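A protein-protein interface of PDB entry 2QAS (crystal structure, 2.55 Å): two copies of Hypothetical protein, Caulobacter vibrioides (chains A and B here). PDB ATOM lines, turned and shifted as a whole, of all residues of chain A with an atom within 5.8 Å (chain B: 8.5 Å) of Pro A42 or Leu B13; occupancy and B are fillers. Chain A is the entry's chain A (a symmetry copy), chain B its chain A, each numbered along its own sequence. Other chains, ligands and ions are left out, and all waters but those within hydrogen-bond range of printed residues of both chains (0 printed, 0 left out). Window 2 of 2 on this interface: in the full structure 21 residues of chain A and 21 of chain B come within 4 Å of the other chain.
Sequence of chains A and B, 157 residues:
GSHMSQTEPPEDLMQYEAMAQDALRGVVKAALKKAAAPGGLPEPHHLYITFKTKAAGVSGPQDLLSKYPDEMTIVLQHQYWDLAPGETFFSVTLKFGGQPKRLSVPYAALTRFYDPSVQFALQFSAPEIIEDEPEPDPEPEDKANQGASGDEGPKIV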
ATOM      1  N   LYS A  34     -30.219   3.580  12.785  1.00  0.00           N
ATOM      2  CA  LYS A  34     -28.898   3.101  13.165  1.00  0.00           C
ATOM      3  C   LYS A  34     -28.215   2.566  11.907  1.00  0.00           C
ATOM      4  O   LYS A  34     -27.000   2.654  11.766  1.00  0.00           O
ATOM      5  CB  LYS A  34     -29.006   1.988  14.212  1.00  0.00           C
ATOM      6  CG  LYS A  34     -29.614   2.436  15.532  1.00  0.00           C
ATOM      7  CD  LYS A  34     -29.522   1.341  16.580  1.00  0.00           C
ATOM      8  CE  LYS A  34     -30.112   1.796  17.912  1.00  0.00           C
ATOM      9  NZ  LYS A  34     -29.887   0.785  18.995  1.00  0.00           N
ATOM     10  N   GLY A  40     -22.991   2.136   8.809  1.00  0.00           N
ATOM     11  CA  GLY A  40     -24.027   1.122   8.751  1.00  0.00           C
ATOM     12  C   GLY A  40     -24.323   0.424  10.063  1.00  0.00           C
ATOM     13  O   GLY A  40     -23.991   0.916  11.140  1.00  0.00           O
ATOM     14  N   LEU A  41     -24.962  -0.735   9.964  1.00  0.00           N
ATOM     15  CA  LEU A  41     -25.319  -1.530  11.129  1.00  0.00           C
ATOM     16  C   LEU A  41     -24.095  -2.186  11.741  1.00  0.00           C
ATOM     17  O   LEU A  41     -23.099  -2.419  11.058  1.00  0.00           O
ATOM     18  CB  LEU A  41     -26.292  -2.641  10.728  1.00  0.00           C
ATOM     19  CG  LEU A  41     -27.700  -2.296  10.253  1.00  0.00           C
ATOM     20  CD1 LEU A  41     -28.259  -3.465   9.460  1.00  0.00           C
ATOM     21  CD2 LEU A  41     -28.582  -1.963  11.443  1.00  0.00           C
ATOM     22  N   PRO A  42     -24.148  -2.486  13.049  1.00  0.00           N
ATOM     23  CA  PRO A  42     -23.008  -3.136  13.699  1.00  0.00           C
ATOM     24  C   PRO A  42     -23.101  -4.621  13.352  1.00  0.00           C
ATOM     25  O   PRO A  42     -24.023  -5.309  13.795  1.00  0.00           O
ATOM     26  CB  PRO A  42     -23.260  -2.868  15.179  1.00  0.00           C
ATOM     27  CG  PRO A  42     -24.758  -2.884  15.262  1.00  0.00           C
ATOM     28  CD  PRO A  42     -25.161  -2.083  14.040  1.00  0.00           C
ATOM     29  N   GLU A  43     -22.168  -5.109  12.541  1.00  0.00           N
ATOM     30  CA  GLU A  43     -22.190  -6.515  12.141  1.00  0.00           C
ATOM     31  C   GLU A  43     -22.237  -7.443  13.352  1.00  0.00           C
ATOM     32  O   GLU A  43     -21.743  -7.102  14.427  1.00  0.00           O
ATOM     33  CB  GLU A  43     -20.976  -6.846  11.268  1.00  0.00           C
ATOM     34  CG  GLU A  43     -19.662  -6.233  11.739  1.00  0.00           C
ATOM     35  CD  GLU A  43     -19.520  -4.772  11.333  1.00  0.00           C
ATOM     36  OE1 GLU A  43     -19.758  -4.475  10.138  1.00  0.00           O
ATOM     37  OE2 GLU A  43     -19.163  -3.928  12.194  1.00  0.00           O
ATOM     38  N   PRO A  44     -22.824  -8.638  13.191  1.00  0.00           N
ATOM     39  CA  PRO A  44     -23.442  -9.195  11.979  1.00  0.00           C
ATOM     40  C   PRO A  44     -24.903  -8.816  11.728  1.00  0.00           C
ATOM     41  O   PRO A  44     -25.593  -9.487  10.964  1.00  0.00           O
ATOM     42  CB  PRO A  44     -23.295 -10.693  12.197  1.00  0.00           C
ATOM     43  CG  PRO A  44     -23.589 -10.805  13.667  1.00  0.00           C
ATOM     44  CD  PRO A  44     -22.766  -9.661  14.253  1.00  0.00           C
ATOM     45  N   HIS A  45     -25.382  -7.753  12.366  1.00  0.00           N
ATOM     46  CA  HIS A  45     -26.774  -7.345  12.190  1.00  0.00           C
ATOM     47  C   HIS A  45     -27.127  -6.904  10.771  1.00  0.00           C
ATOM     48  O   HIS A  45     -26.391  -6.150  10.139  1.00  0.00           O
ATOM     49  CB  HIS A  45     -27.117  -6.212  13.161  1.00  0.00           C
ATOM     50  CG  HIS A  45     -27.142  -6.633  14.597  1.00  0.00           C
ATOM     51  ND1 HIS A  45     -28.203  -7.311  15.155  1.00  0.00           N
ATOM     52  CD2 HIS A  45     -26.229  -6.482  15.586  1.00  0.00           C
ATOM     53  CE1 HIS A  45     -27.945  -7.561  16.426  1.00  0.00           C
ATOM     54  NE2 HIS A  45     -26.753  -7.068  16.712  1.00  0.00           N
ATOM     55  N   VAL A 118     -29.907 -12.118  15.696  1.00  0.00           N
ATOM     56  CA  VAL A 118     -30.355 -12.310  17.070  1.00  0.00           C
ATOM     57  C   VAL A 118     -31.778 -12.845  17.029  1.00  0.00           C
ATOM     58  O   VAL A 118     -32.496 -12.826  18.020  1.00  0.00           O
ATOM     59  CB  VAL A 118     -30.312 -10.977  17.863  1.00  0.00           C
ATOM     60  CG1 VAL A 118     -28.868 -10.528  18.046  1.00  0.00           C
ATOM     61  CG2 VAL A 118     -31.095  -9.892  17.117  1.00  0.00           C
ATOM     62  N   PRO B  10     -26.612 -14.558  21.620  1.00  0.00           N
ATOM     63  CA  PRO B  10     -25.753 -13.519  21.037  1.00  0.00           C
ATOM     64  C   PRO B  10     -26.022 -12.119  21.614  1.00  0.00           C
ATOM     65  O   PRO B  10     -27.179 -11.725  21.796  1.00  0.00           O
ATOM     66  CB  PRO B  10     -26.093 -13.607  19.555  1.00  0.00           C
ATOM     67  CG  PRO B  10     -27.577 -13.826  19.597  1.00  0.00           C
ATOM     68  CD  PRO B  10     -27.774 -14.818  20.744  1.00  0.00           C
ATOM     69  N   GLU B  11     -24.953 -11.380  21.907  1.00  0.00           N
ATOM     70  CA  GLU B  11     -25.084 -10.025  22.441  1.00  0.00           C
ATOM     71  C   GLU B  11     -25.794  -9.155  21.397  1.00  0.00           C
ATOM     72  O   GLU B  11     -25.378  -9.098  20.236  1.00  0.00           O
ATOM     73  CB  GLU B  11     -23.704  -9.429  22.754  1.00  0.00           C
ATOM     74  CG  GLU B  11     -22.856 -10.229  23.751  1.00  0.00           C
ATOM     75  CD  GLU B  11     -22.268 -11.508  23.156  1.00  0.00           C
ATOM     76  OE1 GLU B  11     -21.542 -11.420  22.142  1.00  0.00           O
ATOM     77  OE2 GLU B  11     -22.524 -12.602  23.708  1.00  0.00           O
ATOM     78  N   ASP B  12     -26.862  -8.480  21.819  1.00  0.00           N
ATOM     79  CA  ASP B  12     -27.660  -7.623  20.938  1.00  0.00           C
ATOM     80  C   ASP B  12     -27.139  -6.185  20.912  1.00  0.00           C
ATOM     81  O   ASP B  12     -27.423  -5.401  21.813  1.00  0.00           O
ATOM     82  CB  ASP B  12     -29.116  -7.622  21.417  1.00  0.00           C
ATOM     83  CG  ASP B  12     -30.087  -7.172  20.348  1.00  0.00           C
ATOM     84  OD1 ASP B  12     -29.717  -6.296  19.539  1.00  0.00           O
ATOM     85  OD2 ASP B  12     -31.225  -7.689  20.330  1.00  0.00           O
ATOM     86  N   LEU B  13     -26.389  -5.835  19.873  1.00  0.00           N
ATOM     87  CA  LEU B  13     -25.841  -4.490  19.762  1.00  0.00           C
ATOM     88  C   LEU B  13     -26.909  -3.513  19.281  1.00  0.00           C
ATOM     89  O   LEU B  13     -26.702  -2.299  19.272  1.00  0.00           O
ATOM     90  CB  LEU B  13     -24.654  -4.474  18.792  1.00  0.00           C
ATOM     91  CG  LEU B  13     -23.606  -5.587  18.920  1.00  0.00           C
ATOM     92  CD1 LEU B  13     -22.397  -5.251  18.056  1.00  0.00           C
ATOM     93  CD2 LEU B  13     -23.186  -5.747  20.373  1.00  0.00           C
ATOM     94  N   MET B  14     -28.050  -4.050  18.872  1.00  0.00           N
ATOM     95  CA  MET B  14     -29.151  -3.216  18.408  1.00  0.00           C
ATOM     96  C   MET B  14     -30.094  -2.892  19.568  1.00  0.00           C
ATOM     97  O   MET B  14     -30.895  -1.959  19.487  1.00  0.00           O
ATOM     98  CB  MET B  14     -29.932  -3.935  17.308  1.00  0.00           C
ATOM     99  CG  MET B  14     -29.164  -4.151  16.032  1.00  0.00           C
ATOM    100  SD  MET B  14     -28.812  -2.603  15.197  1.00  0.00           S
ATOM    101  CE  MET B  14     -30.316  -2.381  14.212  1.00  0.00           C
ATOM    102  N   GLN B  15     -29.994  -3.670  20.646  1.00  0.00           N
ATOM    103  CA  GLN B  15     -30.842  -3.474  21.816  1.00  0.00           C
ATOM    104  C   GLN B  15     -32.293  -3.439  21.362  1.00  0.00           C
ATOM    105  O   GLN B  15     -33.036  -2.506  21.672  1.00  0.00           O
ATOM    106  CB  GLN B  15     -30.499  -2.156  22.503  1.00  0.00           C
ATOM    107  CG  GLN B  15     -29.020  -1.942  22.740  1.00  0.00           C
ATOM    108  CD  GLN B  15     -28.739  -0.592  23.377  1.00  0.00           C
ATOM    109  OE1 GLN B  15     -29.163  -0.330  24.507  1.00  0.00           O
ATOM    110  NE2 GLN B  15     -28.033   0.277  22.652  1.00  0.00           N
ATOM    111  N   TYR B  16     -32.697  -4.455  20.615  1.00  0.00           N
ATOM    112  CA  TYR B  16     -34.056  -4.509  20.122  1.00  0.00           C
ATOM    113  C   TYR B  16     -35.046  -4.516  21.270  1.00  0.00           C
ATOM    114  O   TYR B  16     -36.065  -3.824  21.226  1.00  0.00           O
ATOM    115  CB  TYR B  16     -34.257  -5.745  19.238  1.00  0.00           C
ATOM    116  CG  TYR B  16     -33.646  -5.598  17.863  1.00  0.00           C
ATOM    117  CD1 TYR B  16     -32.662  -6.481  17.412  1.00  0.00           C
ATOM    118  CD2 TYR B  16     -34.057  -4.573  17.006  1.00  0.00           C
ATOM    119  CE1 TYR B  16     -32.104  -6.345  16.135  1.00  0.00           C
ATOM    120  CE2 TYR B  16     -33.506  -4.431  15.729  1.00  0.00           C
ATOM    121  CZ  TYR B  16     -32.531  -5.322  15.302  1.00  0.00           C
ATOM    122  OH  TYR B  16     -31.987  -5.186  14.046  1.00  0.00           O
ATOM    123  N   MET B  19     -35.493  -1.064  22.667  1.00  0.00           N
ATOM    124  CA  MET B  19     -36.249  -0.221  21.738  1.00  0.00           C
ATOM    125  C   MET B  19     -37.730  -0.589  21.736  1.00  0.00           C
ATOM    126  O   MET B  19     -38.589   0.263  21.521  1.00  0.00           O
ATOM    127  CB  MET B  19     -35.703  -0.355  20.314  1.00  0.00           C
ATOM    128  CG  MET B  19     -34.283   0.135  20.105  1.00  0.00           C
ATOM    129  SD  MET B  19     -33.749  -0.243  18.417  1.00  0.00           S
ATOM    130  CE  MET B  19     -33.442   1.360  17.800  1.00  0.00           C
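The backbone NH (N) of Leu B13 lies within hydrogen-bond range of a ring nitrogen (NE2) of His A45 (3.4 Å).
The side-chain amino group of Lys A34 lies within hydrogen-bond range of the backbone carbonyl oxygen of Met B14.
OD1 of Asp B12 is in hydrogen-bond range of N of Met B14, at 2.9 Å.
N of Gln B15 sits at hydrogen-bond distance from OD1 of Asp B12, at 2.9 Å.
Among the printed residues, merely in contact across the chains: Leu A41 with Met B14, Lys A34 with Met B19, His A45 with Met B14, Val A118 with Tyr B16, His A45 with Asp B12, Pro A42 with Leu B13, Pro A42 with Met B14, Val A118 with Pro B10 and Val A118 with Asp B12.
Printed residues of chain B within 4 Å of Lys A34: Met B14 and Met B19.
Of the printed residues of chain B, Leu A41 touches Met B14.
Pro A42 touches just these residues of chain B: Leu B13 and Met B14.
Of the printed residues of chain A, Pro B10 touches Val A118.
The nearest residue of chain A that does not touch Leu B13 is Glu A43 (4.1 Å).
The nearest printed residue of chain B that does not touch Lys A34 is Gln B15 (4.1 Å).
Of the 8 printed residues of chain A, 5 touch a printed residue of chain B.
Printed residues of chain A that touch a printed residue of chain B: Lys A34, Leu A41, Pro A42, His A45 and Val A118.
Hydrophobic or aromatic side chains of chain A that line the printed part of chain B: Leu A41, Pro A42, His A45 and Val A118.
Along chain A the printed residues that touch a printed residue of chain B span positions 34 to 118.
Printed residues of chain B that touch a printed residue of chain A: Pro B10, Asp B12, Leu B13, Met B14, Tyr B16 and Met B19.
Among the printed residues, 11 pairs touch across the chains.
No position is printed for both chains.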
